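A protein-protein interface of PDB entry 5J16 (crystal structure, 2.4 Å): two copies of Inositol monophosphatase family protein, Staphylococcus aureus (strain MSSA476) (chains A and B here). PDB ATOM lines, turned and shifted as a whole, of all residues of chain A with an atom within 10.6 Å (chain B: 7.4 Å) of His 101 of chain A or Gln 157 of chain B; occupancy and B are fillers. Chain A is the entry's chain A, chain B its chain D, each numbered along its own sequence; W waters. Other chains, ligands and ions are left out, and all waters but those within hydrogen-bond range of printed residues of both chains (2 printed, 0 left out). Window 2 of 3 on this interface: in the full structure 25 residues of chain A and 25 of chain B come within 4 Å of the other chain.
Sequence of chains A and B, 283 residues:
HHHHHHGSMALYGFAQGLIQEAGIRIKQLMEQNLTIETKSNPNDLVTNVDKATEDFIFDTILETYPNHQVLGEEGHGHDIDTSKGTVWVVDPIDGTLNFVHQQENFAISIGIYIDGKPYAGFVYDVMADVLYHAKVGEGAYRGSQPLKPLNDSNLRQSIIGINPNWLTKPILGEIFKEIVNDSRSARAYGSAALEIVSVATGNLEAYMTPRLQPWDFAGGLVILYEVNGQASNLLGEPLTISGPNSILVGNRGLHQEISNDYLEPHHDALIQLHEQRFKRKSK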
ATOM      1  N   MET A  30     -22.078 -31.567  22.487  1.00  0.00           N
ATOM      2  CA  MET A  30     -21.289 -30.317  22.397  1.00  0.00           C
ATOM      3  C   MET A  30     -19.854 -30.455  22.916  1.00  0.00           C
ATOM      4  O   MET A  30     -18.931 -30.058  22.216  1.00  0.00           O
ATOM      5  CB  MET A  30     -21.947 -29.198  23.232  1.00  0.00           C
ATOM      6  CG  MET A  30     -23.257 -28.636  22.715  1.00  0.00           C
ATOM      7  SD  MET A  30     -24.023 -27.603  23.984  1.00  0.00           S
ATOM      8  CE  MET A  30     -23.612 -25.977  23.382  1.00  0.00           C
ATOM      9  N   VAL A  49     -28.063 -32.334  15.716  1.00  0.00           N
ATOM     10  CA  VAL A  49     -28.331 -32.159  17.134  1.00  0.00           C
ATOM     11  C   VAL A  49     -29.816 -31.810  17.462  1.00  0.00           C
ATOM     12  O   VAL A  49     -30.350 -32.333  18.434  1.00  0.00           O
ATOM     13  CB  VAL A  49     -27.311 -31.176  17.765  1.00  0.00           C
ATOM     14  CG1 VAL A  49     -27.401 -29.782  17.135  1.00  0.00           C
ATOM     15  CG2 VAL A  49     -27.475 -31.119  19.275  1.00  0.00           C
ATOM     16  N   ILE A  93     -34.439 -27.281  20.249  1.00  0.00           N
ATOM     17  CA  ILE A  93     -33.471 -26.172  20.452  1.00  0.00           C
ATOM     18  C   ILE A  93     -34.109 -24.920  19.870  1.00  0.00           C
ATOM     19  O   ILE A  93     -34.129 -24.758  18.655  1.00  0.00           O
ATOM     20  CB  ILE A  93     -32.071 -26.381  19.764  1.00  0.00           C
ATOM     21  CG1 ILE A  93     -31.221 -27.437  20.497  1.00  0.00           C
ATOM     22  CG2 ILE A  93     -31.250 -25.090  19.748  1.00  0.00           C
ATOM     23  CD1 ILE A  93     -31.299 -28.826  19.912  1.00  0.00           C
ATOM     24  N   GLY A  95     -33.599 -21.123  19.430  1.00  0.00           N
ATOM     25  CA  GLY A  95     -32.407 -20.339  19.299  1.00  0.00           C
ATOM     26  C   GLY A  95     -31.252 -21.121  18.720  1.00  0.00           C
ATOM     27  O   GLY A  95     -30.175 -21.150  19.330  1.00  0.00           O
ATOM     28  N   THR A  96     -31.441 -21.754  17.560  1.00  0.00           N
ATOM     29  CA  THR A  96     -30.315 -22.484  16.930  1.00  0.00           C
ATOM     30  C   THR A  96     -29.172 -21.596  16.461  1.00  0.00           C
ATOM     31  O   THR A  96     -28.029 -22.019  16.495  1.00  0.00           O
ATOM     32  CB  THR A  96     -30.713 -23.422  15.754  1.00  0.00           C
ATOM     33  OG1 THR A  96     -31.857 -22.901  15.094  1.00  0.00           O
ATOM     34  CG2 THR A  96     -31.042 -24.788  16.256  1.00  0.00           C
ATOM     35  N   LEU A  97     -29.469 -20.379  16.029  1.00  0.00           N
ATOM     36  CA  LEU A  97     -28.411 -19.436  15.665  1.00  0.00           C
ATOM     37  C   LEU A  97     -27.588 -19.121  16.903  1.00  0.00           C
ATOM     38  O   LEU A  97     -26.379 -19.183  16.864  1.00  0.00           O
ATOM     39  CB  LEU A  97     -28.977 -18.158  15.065  1.00  0.00           C
ATOM     40  CG  LEU A  97     -29.289 -18.311  13.594  1.00  0.00           C
ATOM     41  CD1 LEU A  97     -30.228 -17.188  13.138  1.00  0.00           C
ATOM     42  CD2 LEU A  97     -27.995 -18.316  12.780  1.00  0.00           C
ATOM     43  N   ASN A  98     -28.251 -18.834  18.018  1.00  0.00           N
ATOM     44  CA  ASN A  98     -27.522 -18.684  19.259  1.00  0.00           C
ATOM     45  C   ASN A  98     -26.774 -19.941  19.619  1.00  0.00           C
ATOM     46  O   ASN A  98     -25.685 -19.855  20.159  1.00  0.00           O
ATOM     47  CB  ASN A  98     -28.433 -18.295  20.401  1.00  0.00           C
ATOM     48  CG  ASN A  98     -28.955 -16.886  20.266  1.00  0.00           C
ATOM     49  OD1 ASN A  98     -28.449 -16.081  19.451  1.00  0.00           O
ATOM     50  ND2 ASN A  98     -30.003 -16.570  21.059  1.00  0.00           N
ATOM     51  N   PHE A  99     -27.375 -21.097  19.375  1.00  0.00           N
ATOM     52  CA  PHE A  99     -26.710 -22.365  19.630  1.00  0.00           C
ATOM     53  C   PHE A  99     -25.378 -22.433  18.890  1.00  0.00           C
ATOM     54  O   PHE A  99     -24.354 -22.627  19.526  1.00  0.00           O
ATOM     55  CB  PHE A  99     -27.591 -23.548  19.215  1.00  0.00           C
ATOM     56  CG  PHE A  99     -26.989 -24.873  19.529  1.00  0.00           C
ATOM     57  CD1 PHE A  99     -27.028 -25.363  20.808  1.00  0.00           C
ATOM     58  CD2 PHE A  99     -26.363 -25.618  18.550  1.00  0.00           C
ATOM     59  CE1 PHE A  99     -26.468 -26.593  21.131  1.00  0.00           C
ATOM     60  CE2 PHE A  99     -25.800 -26.848  18.854  1.00  0.00           C
ATOM     61  CZ  PHE A  99     -25.857 -27.334  20.151  1.00  0.00           C
ATOM     62  N   VAL A 100     -25.423 -22.204  17.571  1.00  0.00           N
ATOM     63  CA  VAL A 100     -24.277 -22.279  16.643  1.00  0.00           C
ATOM     64  C   VAL A 100     -23.243 -21.189  16.978  1.00  0.00           C
ATOM     65  O   VAL A 100     -22.043 -21.444  17.122  1.00  0.00           O
ATOM     66  CB  VAL A 100     -24.779 -22.128  15.155  1.00  0.00           C
ATOM     67  CG1 VAL A 100     -23.642 -21.903  14.147  1.00  0.00           C
ATOM     68  CG2 VAL A 100     -25.627 -23.339  14.718  1.00  0.00           C
ATOM     69  N   HIS A 101     -23.707 -19.960  17.108  1.00  0.00           N
ATOM     70  CA  HIS A 101     -22.792 -18.811  17.220  1.00  0.00           C
ATOM     71  C   HIS A 101     -22.296 -18.462  18.609  1.00  0.00           C
ATOM     72  O   HIS A 101     -21.227 -17.857  18.724  1.00  0.00           O
ATOM     73  CB  HIS A 101     -23.428 -17.596  16.613  1.00  0.00           C
ATOM     74  CG  HIS A 101     -23.540 -17.679  15.132  1.00  0.00           C
ATOM     75  ND1 HIS A 101     -22.799 -16.882  14.296  1.00  0.00           N
ATOM     76  CD2 HIS A 101     -24.263 -18.501  14.343  1.00  0.00           C
ATOM     77  CE1 HIS A 101     -23.072 -17.207  13.046  1.00  0.00           C
ATOM     78  NE2 HIS A 101     -23.956 -18.187  13.048  1.00  0.00           N
ATOM     79  N   GLN A 102     -23.062 -18.808  19.652  1.00  0.00           N
ATOM     80  CA  GLN A 102     -22.735 -18.392  21.022  1.00  0.00           C
ATOM     81  C   GLN A 102     -22.517 -19.522  21.994  1.00  0.00           C
ATOM     82  O   GLN A 102     -22.028 -19.302  23.088  1.00  0.00           O
ATOM     83  CB  GLN A 102     -23.842 -17.474  21.552  1.00  0.00           C
ATOM     84  CG  GLN A 102     -24.367 -16.461  20.525  1.00  0.00           C
ATOM     85  CD  GLN A 102     -25.282 -15.444  21.158  1.00  0.00           C
ATOM     86  OE1 GLN A 102     -26.133 -15.790  21.976  1.00  0.00           O
ATOM     87  NE2 GLN A 102     -25.109 -14.166  20.794  1.00  0.00           N
ATOM     88  N   GLN A 103     -22.899 -20.737  21.609  1.00  0.00           N
ATOM     89  CA  GLN A 103     -22.883 -21.885  22.501  1.00  0.00           C
ATOM     90  C   GLN A 103     -23.685 -21.645  23.805  1.00  0.00           C
ATOM     91  O   GLN A 103     -23.431 -22.295  24.809  1.00  0.00           O
ATOM     92  CB  GLN A 103     -21.437 -22.371  22.760  1.00  0.00           C
ATOM     93  CG  GLN A 103     -20.664 -22.779  21.513  1.00  0.00           C
ATOM     94  CD  GLN A 103     -20.194 -21.566  20.675  1.00  0.00           C
ATOM     95  OE1 GLN A 103     -19.587 -20.633  21.199  1.00  0.00           O
ATOM     96  NE2 GLN A 103     -20.535 -21.557  19.369  1.00  0.00           N
ATOM     97  N   GLU A 104     -24.700 -20.776  23.745  1.00  0.00           N
ATOM     98  CA  GLU A 104     -25.555 -20.462  24.894  1.00  0.00           C
ATOM     99  C   GLU A 104     -26.767 -19.664  24.420  1.00  0.00           C
ATOM    100  O   GLU A 104     -26.899 -19.395  23.234  1.00  0.00           O
ATOM    101  CB  GLU A 104     -24.760 -19.697  25.978  1.00  0.00           C
ATOM    102  CG  GLU A 104     -24.150 -18.384  25.489  1.00  0.00           C
ATOM    103  CD  GLU A 104     -23.477 -17.539  26.572  1.00  0.00           C
ATOM    104  OE1 GLU A 104     -23.075 -16.388  26.235  1.00  0.00           O
ATOM    105  OE2 GLU A 104     -23.352 -17.998  27.735  1.00  0.00           O
ATOM    106  N   ASN A 105     -27.633 -19.278  25.361  1.00  0.00           N
ATOM    107  CA  ASN A 105     -28.856 -18.512  25.085  1.00  0.00           C
ATOM    108  C   ASN A 105     -29.822 -19.262  24.148  1.00  0.00           C
ATOM    109  O   ASN A 105     -30.461 -18.642  23.292  1.00  0.00           O
ATOM    110  CB  ASN A 105     -28.506 -17.125  24.516  1.00  0.00           C
ATOM    111  CG  ASN A 105     -27.493 -16.374  25.372  1.00  0.00           C
ATOM    112  OD1 ASN A 105     -27.590 -16.350  26.583  1.00  0.00           O
ATOM    113  ND2 ASN A 105     -26.545 -15.745  24.743  1.00  0.00           N
ATOM    114  N   PHE A 106     -29.925 -20.587  24.321  1.00  0.00           N
ATOM    115  CA  PHE A 106     -30.902 -21.401  23.618  1.00  0.00           C
ATOM    116  C   PHE A 106     -31.636 -22.196  24.652  1.00  0.00           C
ATOM    117  O   PHE A 106     -31.109 -22.429  25.730  1.00  0.00           O
ATOM    118  CB  PHE A 106     -30.266 -22.353  22.573  1.00  0.00           C
ATOM    119  CG  PHE A 106     -29.239 -23.289  23.142  1.00  0.00           C
ATOM    120  CD1 PHE A 106     -29.616 -24.543  23.644  1.00  0.00           C
ATOM    121  CD2 PHE A 106     -27.911 -22.919  23.196  1.00  0.00           C
ATOM    122  CE1 PHE A 106     -28.677 -25.431  24.174  1.00  0.00           C
ATOM    123  CE2 PHE A 106     -26.968 -23.790  23.762  1.00  0.00           C
ATOM    124  CZ  PHE A 106     -27.356 -25.062  24.233  1.00  0.00           C
ATOM    125  N   MET A 127     -27.669 -23.983  28.975  1.00  0.00           N
ATOM    126  CA  MET A 127     -26.335 -23.578  29.425  1.00  0.00           C
ATOM    127  C   MET A 127     -26.327 -22.711  30.693  1.00  0.00           C
ATOM    128  O   MET A 127     -25.316 -22.688  31.404  1.00  0.00           O
ATOM    129  CB  MET A 127     -25.556 -22.897  28.308  1.00  0.00           C
ATOM    130  CG  MET A 127     -25.463 -23.716  27.022  1.00  0.00           C
ATOM    131  SD  MET A 127     -24.890 -25.404  27.184  1.00  0.00           S
ATOM    132  CE  MET A 127     -23.292 -25.029  27.942  1.00  0.00           C
ATOM    133  N   TYR A 189     -32.871 -10.925  21.791  1.00  0.00           N
ATOM    134  CA  TYR A 189     -32.062 -11.991  22.351  1.00  0.00           C
ATOM    135  C   TYR A 189     -31.944 -13.194  21.438  1.00  0.00           C
ATOM    136  O   TYR A 189     -31.051 -14.029  21.630  1.00  0.00           O
ATOM    137  CB  TYR A 189     -32.609 -12.360  23.750  1.00  0.00           C
ATOM    138  CG  TYR A 189     -32.632 -11.149  24.730  1.00  0.00           C
ATOM    139  CD1 TYR A 189     -31.495 -10.380  24.945  1.00  0.00           C
ATOM    140  CD2 TYR A 189     -33.771 -10.818  25.448  1.00  0.00           C
ATOM    141  CE1 TYR A 189     -31.499  -9.314  25.825  1.00  0.00           C
ATOM    142  CE2 TYR A 189     -33.785  -9.755  26.327  1.00  0.00           C
ATOM    143  CZ  TYR A 189     -32.642  -9.004  26.510  1.00  0.00           C
ATOM    144  OH  TYR A 189     -32.626  -7.941  27.387  1.00  0.00           O
ATOM    145  N   GLY A 190     -32.786 -13.302  20.422  1.00  0.00           N
ATOM    146  CA  GLY A 190     -32.691 -14.443  19.517  1.00  0.00           C
ATOM    147  C   GLY A 190     -33.231 -15.767  20.047  1.00  0.00           C
ATOM    148  O   GLY A 190     -32.828 -16.852  19.555  1.00  0.00           O
ATOM    149  N   SER B 153     -15.166 -13.326   9.647  1.00  0.00           N
ATOM    150  CA  SER B 153     -16.449 -13.874   9.241  1.00  0.00           C
ATOM    151  C   SER B 153     -17.007 -13.059   8.081  1.00  0.00           C
ATOM    152  O   SER B 153     -16.626 -11.913   7.859  1.00  0.00           O
ATOM    153  CB  SER B 153     -17.423 -13.860  10.433  1.00  0.00           C
ATOM    154  OG  SER B 153     -17.770 -12.527  10.762  1.00  0.00           O
ATOM    155  N   ASN B 154     -17.910 -13.654   7.341  1.00  0.00           N
ATOM    156  CA  ASN B 154     -18.709 -12.911   6.374  1.00  0.00           C
ATOM    157  C   ASN B 154     -19.999 -12.424   7.024  1.00  0.00           C
ATOM    158  O   ASN B 154     -20.671 -13.175   7.733  1.00  0.00           O
ATOM    159  CB  ASN B 154     -19.031 -13.808   5.173  1.00  0.00           C
ATOM    160  CG  ASN B 154     -17.769 -14.333   4.501  1.00  0.00           C
ATOM    161  OD1 ASN B 154     -16.767 -13.639   4.390  1.00  0.00           O
ATOM    162  ND2 ASN B 154     -17.812 -15.550   4.083  1.00  0.00           N
ATOM    163  N   LEU B 155     -20.360 -11.183   6.741  1.00  0.00           N
ATOM    164  CA  LEU B 155     -21.614 -10.632   7.208  1.00  0.00           C
ATOM    165  C   LEU B 155     -22.788 -11.589   7.118  1.00  0.00           C
ATOM    166  O   LEU B 155     -23.523 -11.747   8.104  1.00  0.00           O
ATOM    167  CB  LEU B 155     -21.984  -9.343   6.492  1.00  0.00           C
ATOM    168  CG  LEU B 155     -23.222  -8.698   7.114  1.00  0.00           C
ATOM    169  CD1 LEU B 155     -22.886  -8.139   8.483  1.00  0.00           C
ATOM    170  CD2 LEU B 155     -23.752  -7.643   6.178  1.00  0.00           C
ATOM    171  N   ARG B 156     -22.958 -12.241   5.980  1.00  0.00           N
ATOM    172  CA  ARG B 156     -24.129 -13.126   5.791  1.00  0.00           C
ATOM    173  C   ARG B 156     -24.149 -14.341   6.751  1.00  0.00           C
ATOM    174  O   ARG B 156     -25.203 -14.939   6.927  1.00  0.00           O
ATOM    175  CB  ARG B 156     -24.284 -13.533   4.311  1.00  0.00           C
ATOM    176  CG  ARG B 156     -23.225 -14.512   3.798  1.00  0.00           C
ATOM    177  CD  ARG B 156     -23.248 -14.791   2.284  1.00  0.00           C
ATOM    178  NE  ARG B 156     -24.584 -15.147   1.758  1.00  0.00           N
ATOM    179  CZ  ARG B 156     -25.233 -16.312   1.944  1.00  0.00           C
ATOM    180  NH1 ARG B 156     -26.447 -16.469   1.415  1.00  0.00           N
ATOM    181  NH2 ARG B 156     -24.708 -17.315   2.664  1.00  0.00           N
ATOM    182  N   GLN B 157     -22.999 -14.694   7.352  1.00  0.00           N
ATOM    183  CA  GLN B 157     -22.930 -15.688   8.464  1.00  0.00           C
ATOM    184  C   GLN B 157     -22.588 -15.003   9.786  1.00  0.00           C
ATOM    185  O   GLN B 157     -21.892 -15.581  10.607  1.00  0.00           O
ATOM    186  CB  GLN B 157     -21.879 -16.788   8.210  1.00  0.00           C
ATOM    187  CG  GLN B 157     -22.325 -17.892   7.269  1.00  0.00           C
ATOM    188  CD  GLN B 157     -22.396 -17.454   5.820  1.00  0.00           C
ATOM    189  OE1 GLN B 157     -23.441 -17.573   5.177  1.00  0.00           O
ATOM    190  NE2 GLN B 157     -21.281 -16.948   5.290  1.00  0.00           N
ATOM    191  N   SER B 158     -23.077 -13.782   9.997  1.00  0.00           N
ATOM    192  CA  SER B 158     -22.713 -13.012  11.180  1.00  0.00           C
ATOM    193  C   SER B 158     -23.942 -12.553  11.945  1.00  0.00           C
ATOM    194  O   SER B 158     -24.951 -12.207  11.346  1.00  0.00           O
ATOM    195  CB  SER B 158     -21.825 -11.830  10.777  1.00  0.00           C
ATOM    196  OG  SER B 158     -20.606 -12.328  10.228  1.00  0.00           O
ATOM    197  N   ILE B 159     -23.847 -12.598  13.273  1.00  0.00           N
ATOM    198  CA  ILE B 159     -24.843 -12.081  14.170  1.00  0.00           C
ATOM    199  C   ILE B 159     -24.323 -10.680  14.581  1.00  0.00           C
ATOM    200  O   ILE B 159     -23.224 -10.544  15.131  1.00  0.00           O
ATOM    201  CB  ILE B 159     -24.968 -12.955  15.429  1.00  0.00           C
ATOM    202  CG1 ILE B 159     -25.146 -14.433  15.083  1.00  0.00           C
ATOM    203  CG2 ILE B 159     -26.161 -12.499  16.274  1.00  0.00           C
ATOM    204  CD1 ILE B 159     -26.522 -14.775  14.541  1.00  0.00           C
ATOM    205  N   ASP B 182     -28.742  -8.191   5.174  1.00  0.00           N
ATOM    206  CA  ASP B 182     -27.735  -9.213   4.790  1.00  0.00           C
ATOM    207  C   ASP B 182     -27.179 -10.045   5.935  1.00  0.00           C
ATOM    208  O   ASP B 182     -26.782 -11.151   5.703  1.00  0.00           O
ATOM    209  CB  ASP B 182     -26.583  -8.576   4.047  1.00  0.00           C
ATOM    210  CG  ASP B 182     -27.058  -7.919   2.792  1.00  0.00           C
ATOM    211  OD1 ASP B 182     -27.531  -8.658   1.901  1.00  0.00           O
ATOM    212  OD2 ASP B 182     -27.041  -6.677   2.731  1.00  0.00           O
ATOM    213  N   SER B 183     -27.112  -9.502   7.152  1.00  0.00           N
ATOM    214  CA  SER B 183     -26.608 -10.257   8.300  1.00  0.00           C
ATOM    215  C   SER B 183     -27.501 -11.467   8.613  1.00  0.00           C
ATOM    216  O   SER B 183     -28.696 -11.455   8.357  1.00  0.00           O
ATOM    217  CB  SER B 183     -26.497  -9.365   9.529  1.00  0.00           C
ATOM    218  OG  SER B 183     -27.784  -9.056  10.016  1.00  0.00           O
ATOM    219  N   ARG B 184     -26.894 -12.517   9.133  1.00  0.00           N
ATOM    220  CA  ARG B 184     -27.608 -13.703   9.547  1.00  0.00           C
ATOM    221  C   ARG B 184     -28.719 -13.415  10.590  1.00  0.00           C
ATOM    222  O   ARG B 184     -29.847 -13.890  10.469  1.00  0.00           O
ATOM    223  CB  ARG B 184     -26.585 -14.715  10.071  1.00  0.00           C
ATOM    224  CG  ARG B 184     -27.080 -16.137  10.127  1.00  0.00           C
ATOM    225  CD  ARG B 184     -27.513 -16.681   8.770  1.00  0.00           C
ATOM    226  NE  ARG B 184     -27.963 -18.051   8.978  1.00  0.00           N
ATOM    227  CZ  ARG B 184     -29.206 -18.436   9.273  1.00  0.00           C
ATOM    228  NH1 ARG B 184     -30.223 -17.569   9.377  1.00  0.00           N
ATOM    229  NH2 ARG B 184     -29.436 -19.733   9.455  1.00  0.00           N
ATOM    230  N   SER B 185     -28.415 -12.611  11.598  1.00  0.00           N
ATOM    231  CA  SER B 185     -29.433 -12.108  12.500  1.00  0.00           C
ATOM    232  C   SER B 185     -28.841 -10.948  13.230  1.00  0.00           C
ATOM    233  O   SER B 185     -27.666 -10.701  13.106  1.00  0.00           O
ATOM    234  CB  SER B 185     -29.863 -13.171  13.532  1.00  0.00           C
ATOM    235  OG  SER B 185     -31.072 -12.768  14.161  1.00  0.00           O
ATOM    236  N   ARG B 187     -29.022  -8.596  17.115  1.00  0.00           N
ATOM    237  CA  ARG B 187     -29.231  -8.675  18.532  1.00  0.00           C
ATOM    238  C   ARG B 187     -29.066  -7.307  19.205  1.00  0.00           C
ATOM    239  O   ARG B 187     -28.388  -6.444  18.685  1.00  0.00           O
ATOM    240  CB  ARG B 187     -28.194  -9.605  19.133  1.00  0.00           C
ATOM    241  CG  ARG B 187     -28.223 -11.025  18.620  1.00  0.00           C
ATOM    242  CD  ARG B 187     -29.337 -11.816  19.294  1.00  0.00           C
ATOM    243  NE  ARG B 187     -29.306 -13.202  18.815  1.00  0.00           N
ATOM    244  CZ  ARG B 187     -29.888 -13.626  17.706  1.00  0.00           C
ATOM    245  NH1 ARG B 187     -30.600 -12.809  16.947  1.00  0.00           N
ATOM    246  NH2 ARG B 187     -29.814 -14.894  17.388  1.00  0.00           N
ATOM    247  N   THR B 201     -15.343 -11.533  22.822  1.00  0.00           N
ATOM    248  CA  THR B 201     -15.503 -12.951  23.193  1.00  0.00           C
ATOM    249  C   THR B 201     -16.107 -13.936  22.133  1.00  0.00           C
ATOM    250  O   THR B 201     -16.299 -15.108  22.438  1.00  0.00           O
ATOM    251  CB  THR B 201     -16.412 -13.098  24.433  1.00  0.00           C
ATOM    252  OG1 THR B 201     -17.703 -12.640  24.086  1.00  0.00           O
ATOM    253  CG2 THR B 201     -15.912 -12.306  25.616  1.00  0.00           C
ATOM    254  N   GLY B 202     -16.440 -13.484  20.929  1.00  0.00           N
ATOM    255  CA  GLY B 202     -17.029 -14.356  19.923  1.00  0.00           C
ATOM    256  C   GLY B 202     -18.547 -14.461  19.909  1.00  0.00           C
ATOM    257  O   GLY B 202     -19.112 -15.143  19.039  1.00  0.00           O
ATOM    258  N   ASN B 203     -19.241 -13.796  20.829  1.00  0.00           N
ATOM    259  CA  ASN B 203     -20.729 -13.885  20.872  1.00  0.00           C
ATOM    260  C   ASN B 203     -21.435 -13.057  19.800  1.00  0.00           C
ATOM    261  O   ASN B 203     -22.481 -13.454  19.314  1.00  0.00           O
ATOM    262  CB  ASN B 203     -21.294 -13.572  22.279  1.00  0.00           C
ATOM    263  CG  ASN B 203     -21.520 -14.854  23.124  1.00  0.00           C
ATOM    264  OD1 ASN B 203     -20.728 -15.831  23.084  1.00  0.00           O
ATOM    265  ND2 ASN B 203     -22.623 -14.863  23.883  1.00  0.00           N
ATOM    266  N   LEU B 204     -20.909 -11.886  19.473  1.00  0.00           N
ATOM    267  CA  LEU B 204     -21.382 -11.129  18.339  1.00  0.00           C
ATOM    268  C   LEU B 204     -20.191 -11.056  17.400  1.00  0.00           C
ATOM    269  O   LEU B 204     -19.060 -11.011  17.858  1.00  0.00           O
ATOM    270  CB  LEU B 204     -21.857  -9.716  18.761  1.00  0.00           C
ATOM    271  CG  LEU B 204     -23.122  -9.608  19.621  1.00  0.00           C
ATOM    272  CD1 LEU B 204     -23.283  -8.192  20.139  1.00  0.00           C
ATOM    273  CD2 LEU B 204     -24.398 -10.037  18.902  1.00  0.00           C
ATOM    274  N   GLU B 205     -20.431 -11.055  16.091  1.00  0.00           N
ATOM    275  CA  GLU B 205     -19.342 -10.881  15.119  1.00  0.00           C
ATOM    276  C   GLU B 205     -19.114  -9.409  14.853  1.00  0.00           C
ATOM    277  O   GLU B 205     -18.019  -9.031  14.448  1.00  0.00           O
ATOM    278  CB  GLU B 205     -19.630 -11.655  13.817  1.00  0.00           C
ATOM    279  CG  GLU B 205     -19.404 -13.176  13.931  1.00  0.00           C
ATOM    280  CD  GLU B 205     -20.536 -13.971  14.609  1.00  0.00           C
ATOM    281  OE1 GLU B 205     -21.716 -13.587  14.482  1.00  0.00           O
ATOM    282  OE2 GLU B 205     -20.265 -15.028  15.241  1.00  0.00           O
ATOM    283  N   LEU B 254     -15.159  -8.910   8.550  1.00  0.00           N
ATOM    284  CA  LEU B 254     -16.481  -8.348   8.437  1.00  0.00           C
ATOM    285  C   LEU B 254     -16.603  -6.842   8.796  1.00  0.00           C
ATOM    286  O   LEU B 254     -17.607  -6.194   8.409  1.00  0.00           O
ATOM    287  CB  LEU B 254     -17.480  -9.223   9.148  1.00  0.00           C
ATOM    288  CG  LEU B 254     -18.239  -8.521  10.219  1.00  0.00           C
ATOM    289  CD1 LEU B 254     -19.554  -9.273  10.346  1.00  0.00           C
ATOM    290  CD2 LEU B 254     -17.336  -8.530  11.451  1.00  0.00           C
ATOM    291  N   GLU B 257     -15.777  -5.452   5.357  1.00  0.00           N
ATOM    292  CA  GLU B 257     -16.951  -5.702   4.550  1.00  0.00           C
ATOM    293  C   GLU B 257     -18.090  -4.733   4.842  1.00  0.00           C
ATOM    294  O   GLU B 257     -18.726  -4.266   3.913  1.00  0.00           O
ATOM    295  CB  GLU B 257     -17.406  -7.151   4.748  1.00  0.00           C
ATOM    296  CG  GLU B 257     -18.599  -7.555   3.908  1.00  0.00           C
ATOM    297  CD  GLU B 257     -19.073  -8.972   4.166  1.00  0.00           C
ATOM    298  OE1 GLU B 257     -20.047  -9.343   3.526  1.00  0.00           O
ATOM    299  OE2 GLU B 257     -18.504  -9.728   4.997  1.00  0.00           O
HETATM  300  O   HOH W   1     -18.576 -17.774  18.743  1.00  0.00           O
HETATM  301  O   HOH W   2     -30.823 -17.622  17.900  1.00  0.00           O
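The side-chain amide oxygen of Asn 98 of chain A sits at hydrogen-bond distance from the guanidinium group of Arg 187 of chain B (2.7 Å). ND1 of His 101 of chain A is in hydrogen-bond range of OE2 of Glu 205 of chain B (3.3 Å). The backbone carbonyl oxygen (O) of Asn 203 of chain B sits at hydrogen-bond distance from the side-chain amide nitrogen (NE2) of Gln 102 of chain A (3.1 Å). The side-chain carboxylate (OE1) of Glu 104 of chain A sits at hydrogen-bond distance from the side-chain amide nitrogen (ND2) of Asn 203 of chain B. The backbone carbonyl oxygen (O) of Tyr 189 of chain A lies within hydrogen-bond range of the guanidinium group (NE) of Arg 187 of chain B, 3.4 Å away. The backbone carbonyl oxygen of His 101 of chain A sits close to the backbone carbonyl oxygen of Gly 202 of chain B, 3.5 Å away.
OE1 of Gln 102 of chain A sits close to OD1 of Asn 98 of chain A, 3.4 Å away. The side-chain amide oxygen (OE1) of Gln 102 of chain A is in hydrogen-bond range of the side-chain amide nitrogen (ND2) of Asn 105 of chain A.
CD2 of Leu 97 of chain A touches CG of Arg 184 of chain B, 3.6 Å away. His 101 of chain A touches Gln 157 of chain B (CE1 to O, 3.2 Å). CG1 of Ile 159 of chain B touches ND1 of His 101 of chain A, 3.5 Å away. Gly 190 of chain A touches Arg 187 of chain B (CA to CZ, 3.4 Å).
His 101 of chain A touches just these residues of chain B: Gln 157 (3.2 Å), Ile 159 (3.5 Å), Gly 202 (3.5 Å) and Glu 205 (3.3 Å). Gln 157 of chain B touches one residue of chain A. No residue of chain A comes within 4 Å of Asn 154 of chain B. Of chain A, only His 101 (3.5 Å) comes within 4 Å of Ile 159 of chain B. Of the printed residues of chain B, Glu 104 of chain A touches Asn 203. Of the printed residues of chain B, Asn 98 of chain A touches Arg 187 (2.7 Å). Printed residues of chain B within 4 Å of Gln 102 of chain A: Asn 203. Val 100 of chain A touches none of the printed residues of chain B. The nearest residue of chain A that does not touch Gln 157 of chain B is Leu 97 of chain A (7.0 Å). The nearest printed residue of chain A that does not touch Glu 205 of chain B is Gln 102 of chain A (6.4 Å).
Of the 19 printed residues of chain B, 7 touch a printed residue of chain A. Hydrophobic or aromatic side chains of chain B within 4 Å of the printed part of chain A: Ile 159. Along chain B the printed residues that touch a printed residue of chain A span positions 157 to 205. Hydrophobic or aromatic side chains of chain A that line the printed part of chain B: Leu 97 and His 101. Among the printed residues, 10 pairs touch across the chains. Among the printed residues, no Asp or Glu carboxylate lies within 4 Å of a Lys or Arg side-chain nitrogen of the other chain.
No position is printed for both chains.
Water W1 bridges O of His 101 of chain A and O of Gly 202 of chain B. Water W2 lies within hydrogen-bond range of O of Gly 190 of chain A (2.7 Å), N of Asn 98 of chain A (2.8 Å) and NH2 of Arg 187 of chain B (3.0 Å).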
